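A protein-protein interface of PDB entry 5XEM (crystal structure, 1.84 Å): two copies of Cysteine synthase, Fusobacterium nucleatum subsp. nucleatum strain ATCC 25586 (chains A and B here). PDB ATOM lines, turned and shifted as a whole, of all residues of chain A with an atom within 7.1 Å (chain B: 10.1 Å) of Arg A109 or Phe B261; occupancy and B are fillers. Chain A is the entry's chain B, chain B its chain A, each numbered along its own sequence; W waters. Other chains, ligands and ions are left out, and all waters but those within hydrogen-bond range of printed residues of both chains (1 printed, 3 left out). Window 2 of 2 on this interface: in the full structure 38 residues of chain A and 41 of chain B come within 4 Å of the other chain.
No position is printed for both chains.
The backbone carbonyl oxygen of Val A87 sits close to the side-chain amide oxygen of Asn B24. OG of Ser B260 is in hydrogen-bond range of O of Ala A110, at 2.7 Å. The backbone carbonyl oxygen of Leu B304 sits close to the side-chain amide oxygen of Gln A106 (3.4 Å).
OE2 of Glu B263 sits at hydrogen-bond distance from N of Asn B24 (2.7 Å). OG of Ser B260 lies within hydrogen-bond range of O of Met B256, 3.5 Å away. O of Ile B265 lies close to N of Ser B260, at 3.2 Å. The backbone NH of Ile B25 sits at hydrogen-bond distance from the side-chain carboxylate of Glu B263 (2.8 Å). The side-chain amide oxygen (OD1) of Asn B24 sits close to the backbone carbonyl oxygen (O) of Lys B262. The backbone carbonyl oxygen (O) of Arg B257 is in hydrogen-bond range of the side-chain hydroxyl (OG) of Ser B260.
Among the printed residues, pairs that only touch across the chains: Ala A110 with Phe B261, Val A87 with Glu B263, Ala A86 with Phe B261, Ala A86 with Ser B260, Arg A109 with Phe B261, Leu A107 with Leu B266, Tyr A111 with Ser B260, Leu A107 with Leu B304, Ala A86 with Lys B262, Gly A112 with Phe B261, Tyr A111 with Leu B266, Tyr A111 with Gly B264, Ala A110 with Leu B266, Met A83 with Gly B264, Tyr A111 with Phe B261 and Ala A86 with Gly B264.
Of the 19 printed residues of chain A, 9 touch a printed residue of chain B. Printed residues of chain A that touch a printed residue of chain B: Met A83, Ala A86, Val A87, Gln A106, Leu A107, Arg A109, Ala A110, Tyr A111 and Gly A112. Hydrophobic or aromatic side chains of chain A that line the printed part of chain B: Met A83, Ala A86, Val A87, Leu A107, Ala A110 and Tyr A111. Of the 18 printed residues of chain B, 8 touch a printed residue of chain A. Hydrophobic or aromatic side chains of chain B within 4 Å of the printed part of chain A: Phe B261, Leu B266 and Leu B304. Among the printed residues, 19 pairs touch across the chains. Among the printed residues, no Asp or Glu carboxylate lies within 4 Å of a Lys or Arg side-chain nitrogen of the other chain.
Arg A109 touches one residue of chain B. Of chain B, only Ser B260 (3.5 Å), Phe B261 (3.4 Å), Lys B262 (3.6 Å) and Gly B264 (3.96 Å) come within 4 Å of Ala A86. Of the printed residues of chain B, Gly A112 touches Phe B261. No residue of chain B comes within 4 Å of Thr A113. Of the printed residues of chain B, Met A83 touches Gly B264 (3.7 Å). Printed residues of chain B within 4 Å of Gln A106: Leu B304. Printed residues of chain A within 4 Å of Glu B263: Val A87. Of the printed residues of chain A, Lys B262 touches Ala A86. Glu B258 touches none of the printed residues of chain A. The nearest residue of chain B that does not touch Arg A109 is Ser B260 (6.1 Å).
Water W1 lies within hydrogen-bond range of the backbone carbonyl oxygen (O) of Gly B264, the side-chain hydroxyl (OH) of Tyr A111 and the backbone NH (N) of Leu B266.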
ATOM      1  N   ALA A  82      13.732  -6.480  19.606  1.00  0.00           N
ATOM      2  CA  ALA A  82      14.336  -5.458  20.479  1.00  0.00           C
ATOM      3  C   ALA A  82      15.622  -4.917  19.883  1.00  0.00           C
ATOM      4  O   ALA A  82      15.840  -3.695  19.822  1.00  0.00           O
ATOM      5  CB  ALA A  82      14.539  -6.010  21.890  1.00  0.00           C
ATOM      6  N   MET A  83      16.467  -5.819  19.381  1.00  0.00           N
ATOM      7  CA  MET A  83      17.724  -5.439  18.765  1.00  0.00           C
ATOM      8  C   MET A  83      17.491  -4.635  17.492  1.00  0.00           C
ATOM      9  O   MET A  83      18.126  -3.602  17.259  1.00  0.00           O
ATOM     10  CB  MET A  83      18.513  -6.713  18.418  1.00  0.00           C
ATOM     11  CG  MET A  83      19.884  -6.442  17.856  1.00  0.00           C
ATOM     12  SD  MET A  83      20.643  -7.965  17.260  1.00  0.00           S
ATOM     13  CE  MET A  83      19.556  -8.356  15.890  1.00  0.00           C
ATOM     14  N   CYS A  85      14.737  -2.955  16.675  1.00  0.00           N
ATOM     15  CA  CYS A  85      14.143  -1.675  17.080  1.00  0.00           C
ATOM     16  C   CYS A  85      15.152  -0.695  17.705  1.00  0.00           C
ATOM     17  O   CYS A  85      15.020   0.529  17.534  1.00  0.00           O
ATOM     18  CB  CYS A  85      12.961  -1.916  18.003  1.00  0.00           C
ATOM     19  SG  CYS A  85      11.518  -2.645  17.163  1.00  0.00           S
ATOM     20  N   ALA A  86      16.188  -1.215  18.380  1.00  0.00           N
ATOM     21  CA  ALA A  86      17.271  -0.375  18.872  1.00  0.00           C
ATOM     22  C   ALA A  86      18.010   0.267  17.688  1.00  0.00           C
ATOM     23  O   ALA A  86      18.225   1.470  17.669  1.00  0.00           O
ATOM     24  CB  ALA A  86      18.247  -1.170  19.758  1.00  0.00           C
ATOM     25  N   VAL A  87      18.338  -0.515  16.677  1.00  0.00           N
ATOM     26  CA  VAL A  87      19.052  -0.016  15.517  1.00  0.00           C
ATOM     27  C   VAL A  87      18.198   0.984  14.745  1.00  0.00           C
ATOM     28  O   VAL A  87      18.716   2.030  14.280  1.00  0.00           O
ATOM     29  CB  VAL A  87      19.422  -1.150  14.567  1.00  0.00           C
ATOM     30  CG1 VAL A  87      19.994  -0.603  13.261  1.00  0.00           C
ATOM     31  CG2 VAL A  87      20.413  -2.090  15.244  1.00  0.00           C
ATOM     32  N   ASN A  89      15.655   2.768  15.933  1.00  0.00           N
ATOM     33  CA  ASN A  89      15.042   3.728  16.841  1.00  0.00           C
ATOM     34  C   ASN A  89      13.500   3.655  16.904  1.00  0.00           C
ATOM     35  O   ASN A  89      12.824   4.689  17.003  1.00  0.00           O
ATOM     36  CB  ASN A  89      15.517   5.162  16.497  1.00  0.00           C
ATOM     37  CG  ASN A  89      15.220   6.152  17.598  1.00  0.00           C
ATOM     38  OD1 ASN A  89      15.233   5.811  18.789  1.00  0.00           O
ATOM     39  ND2 ASN A  89      14.955   7.401  17.211  1.00  0.00           N
ATOM     40  N   GLU A 103      16.635 -14.324  32.003  1.00  0.00           N
ATOM     41  CA  GLU A 103      17.637 -13.793  31.091  1.00  0.00           C
ATOM     42  C   GLU A 103      17.014 -13.232  29.821  1.00  0.00           C
ATOM     43  O   GLU A 103      17.594 -12.348  29.207  1.00  0.00           O
ATOM     44  CB  GLU A 103      18.715 -14.834  30.695  1.00  0.00           C
ATOM     45  CG  GLU A 103      19.667 -15.274  31.811  1.00  0.00           C
ATOM     46  CD  GLU A 103      19.200 -16.544  32.493  1.00  0.00           C
ATOM     47  OE1 GLU A 103      17.998 -16.603  32.826  1.00  0.00           O
ATOM     48  OE2 GLU A 103      20.010 -17.487  32.655  1.00  0.00           O
ATOM     49  N   ARG A 104      15.860 -13.747  29.416  1.00  0.00           N
ATOM     50  CA  ARG A 104      15.193 -13.220  28.212  1.00  0.00           C
ATOM     51  C   ARG A 104      14.792 -11.786  28.480  1.00  0.00           C
ATOM     52  O   ARG A 104      14.953 -10.918  27.627  1.00  0.00           O
ATOM     53  CB  ARG A 104      13.931 -13.981  27.875  1.00  0.00           C
ATOM     54  CG  ARG A 104      14.125 -15.318  27.226  1.00  0.00           C
ATOM     55  CD  ARG A 104      12.921 -16.206  27.495  1.00  0.00           C
ATOM     56  NE  ARG A 104      12.787 -17.217  26.458  1.00  0.00           N
ATOM     57  CZ  ARG A 104      13.623 -18.241  26.292  1.00  0.00           C
ATOM     58  NH1 ARG A 104      14.654 -18.390  27.119  1.00  0.00           N
ATOM     59  NH2 ARG A 104      13.438 -19.111  25.285  1.00  0.00           N
ATOM     60  N   ILE A 105      14.229 -11.570  29.670  1.00  0.00           N
ATOM     61  CA  ILE A 105      13.880 -10.238  30.094  1.00  0.00           C
ATOM     62  C   ILE A 105      15.108  -9.347  30.171  1.00  0.00           C
ATOM     63  O   ILE A 105      15.035  -8.221  29.731  1.00  0.00           O
ATOM     64  CB  ILE A 105      13.208 -10.218  31.474  1.00  0.00           C
ATOM     65  CG1 ILE A 105      11.825 -10.866  31.418  1.00  0.00           C
ATOM     66  CG2 ILE A 105      13.105  -8.796  32.001  1.00  0.00           C
ATOM     67  CD1 ILE A 105      11.274 -11.148  32.805  1.00  0.00           C
ATOM     68  N   GLN A 106      16.224  -9.832  30.718  1.00  0.00           N
ATOM     69  CA  GLN A 106      17.484  -9.078  30.837  1.00  0.00           C
ATOM     70  C   GLN A 106      17.922  -8.533  29.469  1.00  0.00           C
ATOM     71  O   GLN A 106      18.382  -7.397  29.300  1.00  0.00           O
ATOM     72  CB  GLN A 106      18.598 -10.018  31.365  1.00  0.00           C
ATOM     73  CG  GLN A 106      18.457 -10.497  32.814  1.00  0.00           C
ATOM     74  CD  GLN A 106      19.437 -11.598  33.183  1.00  0.00           C
ATOM     75  OE1 GLN A 106      20.460 -11.789  32.521  1.00  0.00           O
ATOM     76  NE2 GLN A 106      19.123 -12.341  34.238  1.00  0.00           N
ATOM     77  N   LEU A 107      17.833  -9.406  28.492  1.00  0.00           N
ATOM     78  CA  LEU A 107      18.282  -9.104  27.128  1.00  0.00           C
ATOM     79  C   LEU A 107      17.386  -8.066  26.464  1.00  0.00           C
ATOM     80  O   LEU A 107      17.873  -7.077  25.918  1.00  0.00           O
ATOM     81  CB  LEU A 107      18.354 -10.377  26.303  1.00  0.00           C
ATOM     82  CG  LEU A 107      19.516 -11.308  26.661  1.00  0.00           C
ATOM     83  CD1 LEU A 107      19.203 -12.735  26.233  1.00  0.00           C
ATOM     84  CD2 LEU A 107      20.817 -10.812  26.011  1.00  0.00           C
ATOM     85  N   MET A 108      16.075  -8.265  26.540  1.00  0.00           N
ATOM     86  CA  MET A 108      15.143  -7.283  25.958  1.00  0.00           C
ATOM     87  C   MET A 108      15.327  -5.895  26.549  1.00  0.00           C
ATOM     88  O   MET A 108      15.390  -4.908  25.812  1.00  0.00           O
ATOM     89  CB  MET A 108      13.687  -7.741  26.120  1.00  0.00           C
ATOM     90  CG  MET A 108      13.305  -8.751  25.064  1.00  0.00           C
ATOM     91  SD  MET A 108      11.592  -9.323  25.189  1.00  0.00           S
ATOM     92  CE  MET A 108      11.800 -10.657  26.357  1.00  0.00           C
ATOM     93  N   ARG A 109      15.437  -5.821  27.875  1.00  0.00           N
ATOM     94  CA  ARG A 109      15.613  -4.521  28.542  1.00  0.00           C
ATOM     95  C   ARG A 109      16.952  -3.837  28.230  1.00  0.00           C
ATOM     96  O   ARG A 109      17.023  -2.611  28.162  1.00  0.00           O
ATOM     97  CB  ARG A 109      15.429  -4.682  30.023  1.00  0.00           C
ATOM     98  CG  ARG A 109      14.014  -5.130  30.341  1.00  0.00           C
ATOM     99  CD  ARG A 109      13.818  -5.095  31.818  1.00  0.00           C
ATOM    100  NE  ARG A 109      13.471  -3.758  32.241  1.00  0.00           N
ATOM    101  CZ  ARG A 109      13.483  -3.349  33.507  1.00  0.00           C
ATOM    102  NH1 ARG A 109      13.867  -4.170  34.468  1.00  0.00           N
ATOM    103  NH2 ARG A 109      13.149  -2.094  33.800  1.00  0.00           N
ATOM    104  N   ALA A 110      17.977  -4.637  27.994  1.00  0.00           N
ATOM    105  CA  ALA A 110      19.302  -4.129  27.560  1.00  0.00           C
ATOM    106  C   ALA A 110      19.183  -3.371  26.254  1.00  0.00           C
ATOM    107  O   ALA A 110      19.879  -2.390  26.041  1.00  0.00           O
ATOM    108  CB  ALA A 110      20.287  -5.269  27.415  1.00  0.00           C
ATOM    109  N   TYR A 111      18.263  -3.788  25.388  1.00  0.00           N
ATOM    110  CA  TYR A 111      18.027  -3.074  24.138  1.00  0.00           C
ATOM    111  C   TYR A 111      16.966  -1.966  24.257  1.00  0.00           C
ATOM    112  O   TYR A 111      16.674  -1.305  23.276  1.00  0.00           O
ATOM    113  CB  TYR A 111      17.598  -4.042  23.051  1.00  0.00           C
ATOM    114  CG  TYR A 111      18.643  -5.052  22.660  1.00  0.00           C
ATOM    115  CD1 TYR A 111      19.814  -4.670  22.024  1.00  0.00           C
ATOM    116  CD2 TYR A 111      18.428  -6.398  22.853  1.00  0.00           C
ATOM    117  CE1 TYR A 111      20.755  -5.619  21.641  1.00  0.00           C
ATOM    118  CE2 TYR A 111      19.368  -7.335  22.478  1.00  0.00           C
ATOM    119  CZ  TYR A 111      20.524  -6.932  21.856  1.00  0.00           C
ATOM    120  OH  TYR A 111      21.473  -7.875  21.499  1.00  0.00           O
ATOM    121  N   GLY A 112      16.415  -1.776  25.453  1.00  0.00           N
ATOM    122  CA  GLY A 112      15.437  -0.705  25.718  1.00  0.00           C
ATOM    123  C   GLY A 112      13.979  -1.060  25.536  1.00  0.00           C
ATOM    124  O   GLY A 112      13.099  -0.180  25.537  1.00  0.00           O
ATOM    125  N   THR A 113      13.705  -2.341  25.413  1.00  0.00           N
ATOM    126  CA  THR A 113      12.342  -2.817  25.254  1.00  0.00           C
ATOM    127  C   THR A 113      11.606  -2.899  26.589  1.00  0.00           C
ATOM    128  O   THR A 113      12.200  -3.230  27.621  1.00  0.00           O
ATOM    129  CB  THR A 113      12.360  -4.148  24.508  1.00  0.00           C
ATOM    130  OG1 THR A 113      12.665  -3.859  23.132  1.00  0.00           O
ATOM    131  CG2 THR A 113      10.990  -4.852  24.636  1.00  0.00           C
ATOM    132  N   GLU A 114      10.327  -2.533  26.575  1.00  0.00           N
ATOM    133  CA  GLU A 114       9.466  -2.651  27.755  1.00  0.00           C
ATOM    134  C   GLU A 114       8.737  -3.974  27.709  1.00  0.00           C
ATOM    135  O   GLU A 114       8.234  -4.398  26.642  1.00  0.00           O
ATOM    136  CB  GLU A 114       8.452  -1.513  27.828  1.00  0.00           C
ATOM    137  CG  GLU A 114       9.065  -0.164  28.050  1.00  0.00           C
ATOM    138  CD  GLU A 114       8.081   0.834  28.607  1.00  0.00           C
ATOM    139  OE1 GLU A 114       7.857   0.838  29.841  1.00  0.00           O
ATOM    140  OE2 GLU A 114       7.529   1.608  27.796  1.00  0.00           O
ATOM    141  N   VAL A 115       8.673  -4.632  28.867  1.00  0.00           N
ATOM    142  CA  VAL A 115       8.124  -5.966  28.973  1.00  0.00           C
ATOM    143  C   VAL A 115       6.914  -5.962  29.895  1.00  0.00           C
ATOM    144  O   VAL A 115       6.971  -5.430  31.010  1.00  0.00           O
ATOM    145  CB  VAL A 115       9.173  -6.967  29.523  1.00  0.00           C
ATOM    146  CG1 VAL A 115       8.551  -8.329  29.805  1.00  0.00           C
ATOM    147  CG2 VAL A 115      10.376  -7.076  28.584  1.00  0.00           C
ATOM    148  N   ASN B  24      24.505   5.806  15.168  1.00  0.00           N
ATOM    149  CA  ASN B  24      23.495   6.543  15.877  1.00  0.00           C
ATOM    150  C   ASN B  24      24.106   7.403  16.959  1.00  0.00           C
ATOM    151  O   ASN B  24      23.690   8.552  17.131  1.00  0.00           O
ATOM    152  CB  ASN B  24      22.423   5.593  16.391  1.00  0.00           C
ATOM    153  CG  ASN B  24      21.724   4.852  15.260  1.00  0.00           C
ATOM    154  OD1 ASN B  24      21.352   3.674  15.386  1.00  0.00           O
ATOM    155  ND2 ASN B  24      21.533   5.548  14.139  1.00  0.00           N
ATOM    156  N   ILE B  25      25.145   6.903  17.628  1.00  0.00           N
ATOM    157  CA  ILE B  25      25.818   7.643  18.675  1.00  0.00           C
ATOM    158  C   ILE B  25      26.724   8.691  18.045  1.00  0.00           C
ATOM    159  O   ILE B  25      27.426   8.398  17.075  1.00  0.00           O
ATOM    160  CB  ILE B  25      26.675   6.699  19.545  1.00  0.00           C
ATOM    161  CG1 ILE B  25      25.789   5.691  20.272  1.00  0.00           C
ATOM    162  CG2 ILE B  25      27.493   7.470  20.565  1.00  0.00           C
ATOM    163  CD1 ILE B  25      26.586   4.634  21.000  1.00  0.00           C
ATOM    164  N   PHE B 253      29.802   1.338  32.373  1.00  0.00           N
ATOM    165  CA  PHE B 253      28.454   0.799  32.422  1.00  0.00           C
ATOM    166  C   PHE B 253      27.504   1.665  31.591  1.00  0.00           C
ATOM    167  O   PHE B 253      26.678   1.146  30.826  1.00  0.00           O
ATOM    168  CB  PHE B 253      27.955   0.673  33.866  1.00  0.00           C
ATOM    169  CG  PHE B 253      28.464  -0.559  34.569  1.00  0.00           C
ATOM    170  CD1 PHE B 253      27.877  -1.794  34.334  1.00  0.00           C
ATOM    171  CD2 PHE B 253      29.551  -0.496  35.407  1.00  0.00           C
ATOM    172  CE1 PHE B 253      28.359  -2.942  34.949  1.00  0.00           C
ATOM    173  CE2 PHE B 253      30.030  -1.636  36.035  1.00  0.00           C
ATOM    174  CZ  PHE B 253      29.441  -2.848  35.814  1.00  0.00           C
ATOM    175  N   GLU B 254      27.632   2.980  31.723  1.00  0.00           N
ATOM    176  CA  GLU B 254      26.769   3.889  30.973  1.00  0.00           C
ATOM    177  C   GLU B 254      26.914   3.673  29.455  1.00  0.00           C
ATOM    178  O   GLU B 254      25.918   3.622  28.713  1.00  0.00           O
ATOM    179  CB  GLU B 254      27.066   5.343  31.368  1.00  0.00           C
ATOM    180  CG  GLU B 254      26.196   6.353  30.634  1.00  0.00           C
ATOM    181  CD  GLU B 254      26.292   7.777  31.187  1.00  0.00           C
ATOM    182  OE1 GLU B 254      26.597   7.955  32.389  1.00  0.00           O
ATOM    183  OE2 GLU B 254      26.036   8.713  30.398  1.00  0.00           O
ATOM    184  N   MET B 255      28.150   3.536  28.990  1.00  0.00           N
ATOM    185  CA  MET B 255      28.424   3.387  27.578  1.00  0.00           C
ATOM    186  C   MET B 255      28.059   1.977  27.082  1.00  0.00           C
ATOM    187  O   MET B 255      27.628   1.836  25.949  1.00  0.00           O
ATOM    188  CB  MET B 255      29.889   3.720  27.281  1.00  0.00           C
ATOM    189  CG  MET B 255      30.199   4.016  25.833  1.00  0.00           C
ATOM    190  SD  MET B 255      29.108   5.221  25.019  1.00  0.00           S
ATOM    191  CE  MET B 255      28.810   6.387  26.347  1.00  0.00           C
ATOM    192  N   MET B 256      28.222   0.959  27.920  1.00  0.00           N
ATOM    193  CA  MET B 256      27.713  -0.384  27.577  1.00  0.00           C
ATOM    194  C   MET B 256      26.208  -0.277  27.271  1.00  0.00           C
ATOM    195  O   MET B 256      25.716  -0.797  26.280  1.00  0.00           O
ATOM    196  CB  MET B 256      27.932  -1.333  28.748  1.00  0.00           C
ATOM    197  CG  MET B 256      27.483  -2.757  28.507  1.00  0.00           C
ATOM    198  SD  MET B 256      27.829  -3.742  29.965  1.00  0.00           S
ATOM    199  CE  MET B 256      26.916  -5.242  29.579  1.00  0.00           C
ATOM    200  N   ARG B 257      25.490   0.418  28.133  1.00  0.00           N
ATOM    201  CA  ARG B 257      24.044   0.590  27.949  1.00  0.00           C
ATOM    202  C   ARG B 257      23.709   1.414  26.705  1.00  0.00           C
ATOM    203  O   ARG B 257      22.765   1.083  25.994  1.00  0.00           O
ATOM    204  CB  ARG B 257      23.397   1.200  29.186  1.00  0.00           C
ATOM    205  CG  ARG B 257      23.381   0.303  30.414  1.00  0.00           C
ATOM    206  CD  ARG B 257      22.691   1.016  31.572  1.00  0.00           C
ATOM    207  NE  ARG B 257      23.080   0.474  32.878  1.00  0.00           N
ATOM    208  CZ  ARG B 257      23.820   1.085  33.807  1.00  0.00           C
ATOM    209  NH1 ARG B 257      24.277   2.325  33.611  1.00  0.00           N
ATOM    210  NH2 ARG B 257      24.092   0.463  34.945  1.00  0.00           N
ATOM    211  N   GLU B 258      24.469   2.471  26.430  1.00  0.00           N
ATOM    212  CA  GLU B 258      24.204   3.319  25.289  1.00  0.00           C
ATOM    213  C   GLU B 258      24.408   2.535  23.991  1.00  0.00           C
ATOM    214  O   GLU B 258      23.636   2.685  23.026  1.00  0.00           O
ATOM    215  CB  GLU B 258      25.102   4.557  25.341  1.00  0.00           C
ATOM    216  CG  GLU B 258      24.653   5.694  24.448  1.00  0.00           C
ATOM    217  CD  GLU B 258      23.355   6.331  24.895  1.00  0.00           C
ATOM    218  OE1 GLU B 258      22.765   5.902  25.911  1.00  0.00           O
ATOM    219  OE2 GLU B 258      22.908   7.262  24.200  1.00  0.00           O
ATOM    220  N   LEU B 259      25.437   1.677  23.961  1.00  0.00           N
ATOM    221  CA  LEU B 259      25.685   0.849  22.772  1.00  0.00           C
ATOM    222  C   LEU B 259      24.506  -0.075  22.469  1.00  0.00           C
ATOM    223  O   LEU B 259      24.120  -0.244  21.313  1.00  0.00           O
ATOM    224  CB  LEU B 259      26.985   0.031  22.927  1.00  0.00           C
ATOM    225  CG  LEU B 259      28.290   0.813  22.702  1.00  0.00           C
ATOM    226  CD1 LEU B 259      29.467   0.075  23.351  1.00  0.00           C
ATOM    227  CD2 LEU B 259      28.527   1.051  21.216  1.00  0.00           C
ATOM    228  N   SER B 260      23.942  -0.693  23.495  1.00  0.00           N
ATOM    229  CA  SER B 260      22.876  -1.635  23.251  1.00  0.00           C
ATOM    230  C   SER B 260      21.609  -0.854  22.907  1.00  0.00           C
ATOM    231  O   SER B 260      20.888  -1.253  21.997  1.00  0.00           O
ATOM    232  CB  SER B 260      22.658  -2.643  24.392  1.00  0.00           C
ATOM    233  OG  SER B 260      22.540  -2.017  25.649  1.00  0.00           O
ATOM    234  N   PHE B 261      21.346   0.239  23.624  1.00  0.00           N
ATOM    235  CA  PHE B 261      20.158   1.085  23.345  1.00  0.00           C
ATOM    236  C   PHE B 261      20.149   1.712  21.975  1.00  0.00           C
ATOM    237  O   PHE B 261      19.103   1.773  21.334  1.00  0.00           O
ATOM    238  CB  PHE B 261      20.054   2.239  24.330  1.00  0.00           C
ATOM    239  CG  PHE B 261      19.642   1.858  25.724  1.00  0.00           C
ATOM    240  CD1 PHE B 261      19.037   0.646  26.020  1.00  0.00           C
ATOM    241  CD2 PHE B 261      19.862   2.765  26.771  1.00  0.00           C
ATOM    242  CE1 PHE B 261      18.649   0.341  27.318  1.00  0.00           C
ATOM    243  CE2 PHE B 261      19.479   2.466  28.078  1.00  0.00           C
ATOM    244  CZ  PHE B 261      18.863   1.248  28.347  1.00  0.00           C
ATOM    245  N   LYS B 262      21.283   2.254  21.550  1.00  0.00           N
ATOM    246  CA  LYS B 262      21.366   3.093  20.339  1.00  0.00           C
ATOM    247  C   LYS B 262      21.905   2.375  19.121  1.00  0.00           C
ATOM    248  O   LYS B 262      21.573   2.747  17.997  1.00  0.00           O
ATOM    249  CB  LYS B 262      22.229   4.333  20.600  1.00  0.00           C
ATOM    250  CG  LYS B 262      21.834   5.148  21.812  1.00  0.00           C
ATOM    251  CD  LYS B 262      20.388   5.616  21.758  1.00  0.00           C
ATOM    252  CE  LYS B 262      20.077   6.557  22.925  1.00  0.00           C
ATOM    253  NZ  LYS B 262      18.626   6.547  23.273  1.00  0.00           N
ATOM    254  N   GLU B 263      22.717   1.337  19.315  1.00  0.00           N
ATOM    255  CA  GLU B 263      23.281   0.604  18.191  1.00  0.00           C
ATOM    256  C   GLU B 263      22.852  -0.861  18.074  1.00  0.00           C
ATOM    257  O   GLU B 263      23.212  -1.531  17.081  1.00  0.00           O
ATOM    258  CB  GLU B 263      24.821   0.676  18.205  1.00  0.00           C
ATOM    259  CG  GLU B 263      25.416   2.073  18.291  1.00  0.00           C
ATOM    260  CD  GLU B 263      25.303   2.884  17.000  1.00  0.00           C
ATOM    261  OE1 GLU B 263      25.290   2.349  15.872  1.00  0.00           O
ATOM    262  OE2 GLU B 263      25.227   4.120  17.109  1.00  0.00           O
ATOM    263  N   GLY B 264      22.141  -1.390  19.066  1.00  0.00           N
ATOM    264  CA  GLY B 264      21.845  -2.829  19.100  1.00  0.00           C
ATOM    265  C   GLY B 264      23.110  -3.685  19.242  1.00  0.00           C
ATOM    266  O   GLY B 264      23.119  -4.857  18.876  1.00  0.00           O
ATOM    267  N   ILE B 265      24.165  -3.123  19.844  1.00  0.00           N
ATOM    268  CA  ILE B 265      25.402  -3.854  20.086  1.00  0.00           C
ATOM    269  C   ILE B 265      25.431  -4.173  21.578  1.00  0.00           C
ATOM    270  O   ILE B 265      25.460  -3.257  22.414  1.00  0.00           O
ATOM    271  CB  ILE B 265      26.649  -3.027  19.709  1.00  0.00           C
ATOM    272  CG1 ILE B 265      26.721  -2.773  18.218  1.00  0.00           C
ATOM    273  CG2 ILE B 265      27.926  -3.691  20.226  1.00  0.00           C
ATOM    274  CD1 ILE B 265      27.719  -1.691  17.824  1.00  0.00           C
ATOM    275  N   LEU B 266      25.442  -5.460  21.901  1.00  0.00           N
ATOM    276  CA  LEU B 266      25.470  -5.915  23.273  1.00  0.00           C
ATOM    277  C   LEU B 266      26.886  -6.393  23.559  1.00  0.00           C
ATOM    278  O   LEU B 266      27.259  -7.527  23.271  1.00  0.00           O
ATOM    279  CB  LEU B 266      24.426  -7.025  23.487  1.00  0.00           C
ATOM    280  CG  LEU B 266      24.227  -7.511  24.928  1.00  0.00           C
ATOM    281  CD1 LEU B 266      23.344  -6.548  25.695  1.00  0.00           C
ATOM    282  CD2 LEU B 266      23.590  -8.894  24.972  1.00  0.00           C
ATOM    283  N   GLY B 267      27.711  -5.498  24.084  1.00  0.00           N
ATOM    284  CA  GLY B 267      29.078  -5.811  24.425  1.00  0.00           C
ATOM    285  C   GLY B 267      29.232  -5.871  25.921  1.00  0.00           C
ATOM    286  O   GLY B 267      28.350  -5.441  26.681  1.00  0.00           O
ATOM    287  N   LEU B 304      24.529  -9.463  32.232  1.00  0.00           N
ATOM    288  CA  LEU B 304      23.171  -8.923  32.406  1.00  0.00           C
ATOM    289  C   LEU B 304      22.434  -9.411  33.653  1.00  0.00           C
ATOM    290  O   LEU B 304      21.398  -8.872  33.977  1.00  0.00           O
ATOM    291  CB  LEU B 304      22.321  -9.198  31.186  1.00  0.00           C
ATOM    292  CG  LEU B 304      22.721  -8.460  29.914  1.00  0.00           C
ATOM    293  CD1 LEU B 304      21.710  -8.740  28.813  1.00  0.00           C
ATOM    294  CD2 LEU B 304      22.869  -6.963  30.158  1.00  0.00           C
HETATM  295  O   HOH W   1      23.866  -7.090  19.853  1.00  0.00           O
